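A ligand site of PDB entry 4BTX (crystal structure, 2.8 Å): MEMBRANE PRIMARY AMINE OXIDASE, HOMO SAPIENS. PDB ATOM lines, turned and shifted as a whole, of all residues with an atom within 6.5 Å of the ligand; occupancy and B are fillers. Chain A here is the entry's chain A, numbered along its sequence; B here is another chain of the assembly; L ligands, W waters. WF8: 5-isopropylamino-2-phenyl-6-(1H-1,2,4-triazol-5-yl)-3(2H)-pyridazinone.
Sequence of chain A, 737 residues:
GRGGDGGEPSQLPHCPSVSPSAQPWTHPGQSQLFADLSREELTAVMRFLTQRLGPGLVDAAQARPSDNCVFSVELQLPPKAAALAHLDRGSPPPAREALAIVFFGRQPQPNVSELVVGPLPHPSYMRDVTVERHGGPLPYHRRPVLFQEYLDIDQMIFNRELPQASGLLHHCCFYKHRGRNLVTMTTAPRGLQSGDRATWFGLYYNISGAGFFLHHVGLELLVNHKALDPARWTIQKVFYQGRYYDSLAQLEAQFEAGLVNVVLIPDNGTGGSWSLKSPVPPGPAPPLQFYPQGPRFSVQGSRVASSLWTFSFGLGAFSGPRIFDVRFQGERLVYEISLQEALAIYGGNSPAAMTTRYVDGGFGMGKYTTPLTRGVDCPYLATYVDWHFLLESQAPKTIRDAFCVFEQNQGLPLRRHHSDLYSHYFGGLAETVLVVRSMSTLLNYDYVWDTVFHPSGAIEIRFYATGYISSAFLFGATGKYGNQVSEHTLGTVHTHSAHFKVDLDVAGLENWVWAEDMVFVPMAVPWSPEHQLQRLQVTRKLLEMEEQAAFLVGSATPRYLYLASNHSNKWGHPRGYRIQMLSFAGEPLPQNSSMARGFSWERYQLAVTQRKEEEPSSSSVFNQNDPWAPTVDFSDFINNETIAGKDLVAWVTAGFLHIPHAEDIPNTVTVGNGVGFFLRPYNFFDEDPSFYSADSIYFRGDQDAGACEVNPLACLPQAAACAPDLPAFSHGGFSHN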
ATOM      1  N   VAL A 145      -9.403  17.168  15.123  1.00  0.00           N
ATOM      2  CA  VAL A 145      -8.984  18.241  14.272  1.00  0.00           C
ATOM      3  C   VAL A 145      -7.584  17.899  13.812  1.00  0.00           C
ATOM      4  O   VAL A 145      -6.729  17.506  14.624  1.00  0.00           O
ATOM      5  CB  VAL A 145      -9.079  19.568  15.059  1.00  0.00           C
ATOM      6  CG1 VAL A 145      -8.377  20.721  14.356  1.00  0.00           C
ATOM      7  CG2 VAL A 145     -10.531  19.918  15.289  1.00  0.00           C
ATOM      8  N   LEU A 146      -7.373  18.026  12.505  1.00  0.00           N
ATOM      9  CA  LEU A 146      -6.093  17.736  11.872  1.00  0.00           C
ATOM     10  C   LEU A 146      -5.147  18.893  11.972  1.00  0.00           C
ATOM     11  O   LEU A 146      -5.558  20.031  12.022  1.00  0.00           O
ATOM     12  CB  LEU A 146      -6.312  17.398  10.378  1.00  0.00           C
ATOM     13  CG  LEU A 146      -7.179  16.135  10.129  1.00  0.00           C
ATOM     14  CD1 LEU A 146      -7.968  16.160   8.804  1.00  0.00           C
ATOM     15  CD2 LEU A 146      -6.311  14.889  10.259  1.00  0.00           C
ATOM     16  N   PHE A 147      -3.854  18.619  11.973  1.00  0.00           N
ATOM     17  CA  PHE A 147      -2.883  19.679  11.749  1.00  0.00           C
ATOM     18  C   PHE A 147      -3.320  20.688  10.655  1.00  0.00           C
ATOM     19  O   PHE A 147      -3.312  21.891  10.896  1.00  0.00           O
ATOM     20  CB  PHE A 147      -1.517  19.071  11.419  1.00  0.00           C
ATOM     21  CG  PHE A 147      -0.930  18.224  12.519  1.00  0.00           C
ATOM     22  CD1 PHE A 147      -1.146  18.513  13.858  1.00  0.00           C
ATOM     23  CD2 PHE A 147      -0.115  17.138  12.200  1.00  0.00           C
ATOM     24  CE1 PHE A 147      -0.582  17.739  14.861  1.00  0.00           C
ATOM     25  CE2 PHE A 147       0.432  16.354  13.192  1.00  0.00           C
ATOM     26  CZ  PHE A 147       0.209  16.656  14.522  1.00  0.00           C
ATOM     27  N   GLN A 148      -3.696  20.217   9.468  1.00  0.00           N
ATOM     28  CA  GLN A 148      -4.221  21.130   8.424  1.00  0.00           C
ATOM     29  C   GLN A 148      -5.349  21.990   8.907  1.00  0.00           C
ATOM     30  O   GLN A 148      -5.356  23.200   8.663  1.00  0.00           O
ATOM     31  CB  GLN A 148      -4.781  20.371   7.211  1.00  0.00           C
ATOM     32  CG  GLN A 148      -3.886  20.399   6.013  1.00  0.00           C
ATOM     33  CD  GLN A 148      -3.389  21.786   5.646  1.00  0.00           C
ATOM     34  OE1 GLN A 148      -4.195  22.718   5.552  1.00  0.00           O
ATOM     35  NE2 GLN A 148      -2.080  21.930   5.409  1.00  0.00           N
ATOM     36  N   TYR A 150      -6.126  22.896  11.840  1.00  0.00           N
ATOM     37  CA  TYR A 150      -5.564  23.958  12.678  1.00  0.00           C
ATOM     38  C   TYR A 150      -4.975  25.095  11.813  1.00  0.00           C
ATOM     39  O   TYR A 150      -5.208  26.275  12.101  1.00  0.00           O
ATOM     40  CB  TYR A 150      -4.531  23.421  13.708  1.00  0.00           C
ATOM     41  CG  TYR A 150      -5.166  22.642  14.845  1.00  0.00           C
ATOM     42  CD1 TYR A 150      -6.165  23.193  15.630  1.00  0.00           C
ATOM     43  CD2 TYR A 150      -4.754  21.342  15.137  1.00  0.00           C
ATOM     44  CE1 TYR A 150      -6.756  22.466  16.668  1.00  0.00           C
ATOM     45  CE2 TYR A 150      -5.341  20.619  16.166  1.00  0.00           C
ATOM     46  CZ  TYR A 150      -6.340  21.167  16.927  1.00  0.00           C
ATOM     47  OH  TYR A 150      -6.905  20.448  17.955  1.00  0.00           O
ATOM     48  N   LEU A 151      -4.257  24.759  10.747  1.00  0.00           N
ATOM     49  CA  LEU A 151      -3.678  25.788   9.879  1.00  0.00           C
ATOM     50  C   LEU A 151      -4.735  26.555   9.099  1.00  0.00           C
ATOM     51  O   LEU A 151      -4.628  27.746   8.992  1.00  0.00           O
ATOM     52  CB  LEU A 151      -2.685  25.202   8.888  1.00  0.00           C
ATOM     53  CG  LEU A 151      -1.460  24.525   9.487  1.00  0.00           C
ATOM     54  CD1 LEU A 151      -0.893  23.576   8.448  1.00  0.00           C
ATOM     55  CD2 LEU A 151      -0.401  25.509   9.950  1.00  0.00           C
ATOM     56  N   ILE A 153      -7.839  27.144   9.938  1.00  0.00           N
ATOM     57  CA  ILE A 153      -8.398  28.014  10.960  1.00  0.00           C
ATOM     58  C   ILE A 153      -7.505  29.231  11.201  1.00  0.00           C
ATOM     59  O   ILE A 153      -7.976  30.363  11.117  1.00  0.00           O
ATOM     60  CB  ILE A 153      -8.540  27.233  12.268  1.00  0.00           C
ATOM     61  CG1 ILE A 153      -9.777  26.325  12.180  1.00  0.00           C
ATOM     62  CG2 ILE A 153      -8.583  28.182  13.458  1.00  0.00           C
ATOM     63  CD1 ILE A 153      -9.909  25.302  13.297  1.00  0.00           C
ATOM     64  N   ASP A 154      -6.236  28.998  11.502  1.00  0.00           N
ATOM     65  CA  ASP A 154      -5.295  30.096  11.738  1.00  0.00           C
ATOM     66  C   ASP A 154      -5.047  31.042  10.558  1.00  0.00           C
ATOM     67  O   ASP A 154      -4.393  32.053  10.725  1.00  0.00           O
ATOM     68  CB  ASP A 154      -3.960  29.534  12.212  1.00  0.00           C
ATOM     69  CG  ASP A 154      -3.986  29.190  13.673  1.00  0.00           C
ATOM     70  OD1 ASP A 154      -5.105  29.022  14.220  1.00  0.00           O
ATOM     71  OD2 ASP A 154      -2.896  29.102  14.273  1.00  0.00           O
ATOM     72  N   THR A 184      -2.403  31.086  18.447  1.00  0.00           N
ATOM     73  CA  THR A 184      -3.632  30.549  19.047  1.00  0.00           C
ATOM     74  C   THR A 184      -3.402  29.254  19.823  1.00  0.00           C
ATOM     75  O   THR A 184      -2.303  28.670  19.795  1.00  0.00           O
ATOM     76  CB  THR A 184      -4.719  30.301  18.002  1.00  0.00           C
ATOM     77  OG1 THR A 184      -4.141  29.657  16.862  1.00  0.00           O
ATOM     78  CG2 THR A 184      -5.308  31.583  17.589  1.00  0.00           C
ATOM     79  N   MET A 185      -4.457  28.828  20.523  1.00  0.00           N
ATOM     80  CA  MET A 185      -4.482  27.561  21.256  1.00  0.00           C
ATOM     81  C   MET A 185      -5.922  27.100  21.419  1.00  0.00           C
ATOM     82  O   MET A 185      -6.823  27.904  21.615  1.00  0.00           O
ATOM     83  CB  MET A 185      -3.786  27.712  22.614  1.00  0.00           C
ATOM     84  CG  MET A 185      -3.943  26.493  23.543  1.00  0.00           C
ATOM     85  SD  MET A 185      -2.735  26.486  24.886  1.00  0.00           S
ATOM     86  CE  MET A 185      -3.850  26.078  26.212  1.00  0.00           C
ATOM     87  N   THR A 186      -6.137  25.803  21.351  1.00  0.00           N
ATOM     88  CA  THR A 186      -7.482  25.262  21.206  1.00  0.00           C
ATOM     89  C   THR A 186      -8.045  24.917  22.546  1.00  0.00           C
ATOM     90  O   THR A 186      -7.334  24.998  23.529  1.00  0.00           O
ATOM     91  CB  THR A 186      -7.502  23.989  20.332  1.00  0.00           C
ATOM     92  OG1 THR A 186      -8.729  23.267  20.514  1.00  0.00           O
ATOM     93  CG2 THR A 186      -6.328  23.081  20.682  1.00  0.00           C
ATOM     94  N   ARG A 190     -16.082  21.304  21.604  1.00  0.00           N
ATOM     95  CA  ARG A 190     -16.145  22.366  20.652  1.00  0.00           C
ATOM     96  C   ARG A 190     -17.627  22.548  20.339  1.00  0.00           C
ATOM     97  O   ARG A 190     -18.178  21.925  19.445  1.00  0.00           O
ATOM     98  CB  ARG A 190     -15.290  22.011  19.428  1.00  0.00           C
ATOM     99  CG  ARG A 190     -14.182  21.002  19.729  1.00  0.00           C
ATOM    100  CD  ARG A 190     -13.293  20.687  18.525  1.00  0.00           C
ATOM    101  NE  ARG A 190     -12.086  21.500  18.536  1.00  0.00           N
ATOM    102  CZ  ARG A 190     -10.850  21.068  18.716  1.00  0.00           C
ATOM    103  NH1 ARG A 190     -10.572  19.774  18.868  1.00  0.00           N
ATOM    104  NH2 ARG A 190      -9.853  21.942  18.730  1.00  0.00           N
ATOM    105  N   PHE A 201     -10.833  29.884  20.786  1.00  0.00           N
ATOM    106  CA  PHE A 201      -9.379  29.975  20.767  1.00  0.00           C
ATOM    107  C   PHE A 201      -8.905  31.229  21.506  1.00  0.00           C
ATOM    108  O   PHE A 201      -9.366  32.337  21.252  1.00  0.00           O
ATOM    109  CB  PHE A 201      -8.840  30.048  19.337  1.00  0.00           C
ATOM    110  CG  PHE A 201      -8.900  28.760  18.579  1.00  0.00           C
ATOM    111  CD1 PHE A 201     -10.072  28.374  17.920  1.00  0.00           C
ATOM    112  CD2 PHE A 201      -7.769  27.946  18.457  1.00  0.00           C
ATOM    113  CE1 PHE A 201     -10.116  27.183  17.199  1.00  0.00           C
ATOM    114  CE2 PHE A 201      -7.813  26.755  17.736  1.00  0.00           C
ATOM    115  CZ  PHE A 201      -8.990  26.376  17.113  1.00  0.00           C
ATOM    116  N   PHE A 363      -6.576  13.880  21.536  1.00  0.00           N
ATOM    117  CA  PHE A 363      -5.364  14.348  20.876  1.00  0.00           C
ATOM    118  C   PHE A 363      -4.361  13.199  20.826  1.00  0.00           C
ATOM    119  O   PHE A 363      -3.743  12.976  19.787  1.00  0.00           O
ATOM    120  CB  PHE A 363      -4.722  15.526  21.634  1.00  0.00           C
ATOM    121  CG  PHE A 363      -5.669  16.662  21.903  1.00  0.00           C
ATOM    122  CD1 PHE A 363      -6.546  17.112  20.918  1.00  0.00           C
ATOM    123  CD2 PHE A 363      -5.672  17.293  23.130  1.00  0.00           C
ATOM    124  CE1 PHE A 363      -7.416  18.162  21.162  1.00  0.00           C
ATOM    125  CE2 PHE A 363      -6.546  18.339  23.382  1.00  0.00           C
ATOM    126  CZ  PHE A 363      -7.414  18.767  22.403  1.00  0.00           C
ATOM    127  N   TYR A 368       1.543  12.406  21.249  1.00  0.00           N
ATOM    128  CA  TYR A 368       2.207  13.592  21.809  1.00  0.00           C
ATOM    129  C   TYR A 368       3.274  13.222  22.808  1.00  0.00           C
ATOM    130  O   TYR A 368       3.709  14.036  23.590  1.00  0.00           O
ATOM    131  CB  TYR A 368       1.197  14.567  22.417  1.00  0.00           C
ATOM    132  CG  TYR A 368       0.372  15.296  21.361  1.00  0.00           C
ATOM    133  CD1 TYR A 368       0.836  16.476  20.775  1.00  0.00           C
ATOM    134  CD2 TYR A 368      -0.868  14.809  20.957  1.00  0.00           C
ATOM    135  CE1 TYR A 368       0.081  17.153  19.810  1.00  0.00           C
ATOM    136  CE2 TYR A 368      -1.618  15.482  20.004  1.00  0.00           C
ATOM    137  CZ  TYR A 368      -1.151  16.646  19.436  1.00  0.00           C
ATOM    138  OH  TYR A 368      -1.932  17.284  18.479  1.00  0.00           O
ATOM    139  N   THR A 441       3.347  15.260  26.326  1.00  0.00           N
ATOM    140  CA  THR A 441       3.384  16.719  26.523  1.00  0.00           C
ATOM    141  C   THR A 441       2.319  17.276  25.664  1.00  0.00           C
ATOM    142  O   THR A 441       2.511  17.394  24.497  1.00  0.00           O
ATOM    143  CB  THR A 441       4.721  17.388  26.145  1.00  0.00           C
ATOM    144  OG1 THR A 441       5.775  16.949  27.026  1.00  0.00           O
ATOM    145  CG2 THR A 441       4.594  18.868  26.266  1.00  0.00           C
ATOM    146  N   LEU A 442       1.158  17.581  26.250  1.00  0.00           N
ATOM    147  CA  LEU A 442       0.058  18.140  25.493  1.00  0.00           C
ATOM    148  C   LEU A 442      -0.185  19.605  25.850  1.00  0.00           C
ATOM    149  O   LEU A 442      -0.454  19.948  27.012  1.00  0.00           O
ATOM    150  CB  LEU A 442      -1.233  17.370  25.720  1.00  0.00           C
ATOM    151  CG  LEU A 442      -1.198  15.962  25.166  1.00  0.00           C
ATOM    152  CD1 LEU A 442      -0.834  14.989  26.277  1.00  0.00           C
ATOM    153  CD2 LEU A 442      -2.543  15.617  24.552  1.00  0.00           C
ATOM    154  N   LEU A 443      -0.137  20.430  24.800  1.00  0.00           N
ATOM    155  CA  LEU A 443      -0.169  21.858  24.930  1.00  0.00           C
ATOM    156  C   LEU A 443       0.823  22.197  26.042  1.00  0.00           C
ATOM    157  O   LEU A 443       2.050  21.975  25.895  1.00  0.00           O
ATOM    158  CB  LEU A 443      -1.587  22.287  25.256  1.00  0.00           C
ATOM    159  CG  LEU A 443      -2.611  21.956  24.169  1.00  0.00           C
ATOM    160  CD1 LEU A 443      -4.013  22.202  24.658  1.00  0.00           C
ATOM    161  CD2 LEU A 443      -2.398  22.780  22.922  1.00  0.00           C
ATOM    162  N   LEU B 421       5.677  22.913  19.893  1.00  0.00           N
ATOM    163  CA  LEU B 421       4.639  23.778  19.362  1.00  0.00           C
ATOM    164  C   LEU B 421       5.176  25.195  19.296  1.00  0.00           C
ATOM    165  O   LEU B 421       5.782  25.683  20.263  1.00  0.00           O
ATOM    166  CB  LEU B 421       3.453  23.749  20.277  1.00  0.00           C
ATOM    167  CG  LEU B 421       2.186  24.381  19.723  1.00  0.00           C
ATOM    168  CD1 LEU B 421       1.767  23.744  18.412  1.00  0.00           C
ATOM    169  CD2 LEU B 421       1.084  24.244  20.771  1.00  0.00           C
ATOM    170  N   TYR B 422       4.991  25.830  18.132  1.00  0.00           N
ATOM    171  CA  TYR B 422       5.416  27.198  17.878  1.00  0.00           C
ATOM    172  C   TYR B 422       6.870  27.535  18.197  1.00  0.00           C
ATOM    173  O   TYR B 422       7.476  28.318  17.494  1.00  0.00           O
ATOM    174  CB  TYR B 422       4.494  28.145  18.606  1.00  0.00           C
ATOM    175  CG  TYR B 422       3.019  27.938  18.333  1.00  0.00           C
ATOM    176  CD1 TYR B 422       2.545  27.716  17.067  1.00  0.00           C
ATOM    177  CD2 TYR B 422       2.087  28.028  19.364  1.00  0.00           C
ATOM    178  CE1 TYR B 422       1.195  27.569  16.804  1.00  0.00           C
ATOM    179  CE2 TYR B 422       0.729  27.883  19.121  1.00  0.00           C
ATOM    180  CZ  TYR B 422       0.283  27.649  17.840  1.00  0.00           C
ATOM    181  OH  TYR B 422      -1.073  27.463  17.593  1.00  0.00           O
HETATM  182  CAG WF8 L   1      -1.364  20.372  20.115  1.00  0.00           C
HETATM  183  CAE WF8 L   1      -1.816  19.749  21.258  1.00  0.00           C
HETATM  184  CAD WF8 L   1      -3.199  19.522  21.392  1.00  0.00           C
HETATM  185  CAF WF8 L   1      -4.096  19.927  20.402  1.00  0.00           C
HETATM  186  CAH WF8 L   1      -3.627  20.557  19.246  1.00  0.00           C
HETATM  187  CAP WF8 L   1      -2.255  20.747  19.091  1.00  0.00           C
HETATM  188  NAV WF8 L   1      -1.751  21.393  18.028  1.00  0.00           N
HETATM  189  NAM WF8 L   1      -2.274  22.518  17.789  1.00  0.00           N
HETATM  190  CAT WF8 L   1      -0.689  20.931  17.296  1.00  0.00           C
HETATM  191  OAC WF8 L   1      -0.160  19.823  17.522  1.00  0.00           O
HETATM  192  CAJ WF8 L   1      -0.226  21.746  16.251  1.00  0.00           C
HETATM  193  CAR WF8 L   1      -0.854  22.977  15.999  1.00  0.00           C
HETATM  194  NAN WF8 L   1      -0.443  23.838  15.043  1.00  0.00           N
HETATM  195  CAU WF8 L   1       0.020  23.537  13.668  1.00  0.00           C
HETATM  196  CAB WF8 L   1       1.542  23.335  13.719  1.00  0.00           C
HETATM  197  CAA WF8 L   1      -0.720  22.362  13.008  1.00  0.00           C
HETATM  198  CAS WF8 L   1      -1.916  23.394  16.828  1.00  0.00           C
HETATM  199  CAQ WF8 L   1      -2.632  24.549  16.751  1.00  0.00           C
HETATM  200  NAK WF8 L   1      -3.395  25.010  17.744  1.00  0.00           N
HETATM  201  CAI WF8 L   1      -3.944  26.130  17.292  1.00  0.00           C
HETATM  202  NAO WF8 L   1      -3.497  26.319  16.069  1.00  0.00           N
HETATM  203  NAL WF8 L   1      -2.750  25.425  15.754  1.00  0.00           N
HETATM  204  O   HOH W   1       2.557  18.886  17.407  1.00  0.00           O
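OH of Tyr 422 of chain B lies within hydrogen-bond range of NAO of the ligand (3.1 Å).
The side-chain hydroxyl (OH) of Tyr 368 sits at hydrogen-bond distance from an oxygen (OAC) of the ligand.
The side-chain carboxylate of Asp 154 is in hydrogen-bond range of a nitrogen (NAO) of the ligand (3.4 Å).
OG1 of Thr 184 is in hydrogen-bond range of NAO of the ligand, at 3.5 Å.
The backbone carbonyl oxygen (O) of Thr 184 lies within hydrogen-bond range of the side-chain hydroxyl (OH) of Tyr 422 of chain B (2.8 Å).
N of Thr 441 lies within hydrogen-bond range of O of Tyr 368 (3.0 Å).
The side-chain carboxylate (OD1) of Asp 154 lies within hydrogen-bond range of the side-chain hydroxyl (OG1) of Thr 184 (2.9 Å).
The side-chain hydroxyl (OH) of Tyr 150 lies within hydrogen-bond range of the guanidinium group (NH2) of Arg 190, 3.4 Å away.
The guanidinium group of Arg 190 sits at hydrogen-bond distance from the side-chain hydroxyl of Thr 186.
Phe 147 touches the ligand (O to CAA, 3.4 Å).
Tyr 150 touches the ligand (CB to NAL, 3.4 Å).
CG2 of Thr 186 touches CAF of the ligand, 3.9 Å away.
Phe 201 touches the ligand.
Phe 363 touches the ligand.
Leu 443 touches the ligand.
Leu 421 of chain B touches the ligand.
Hydrophobic or aromatic side chains that line the ligand: Phe 147, Tyr 150, Phe 201, Phe 363, Tyr 368, Leu 443 and Leu 421 of chain B.
Along chain A the residues within 4 Å of the ligand span positions 147 to 443.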
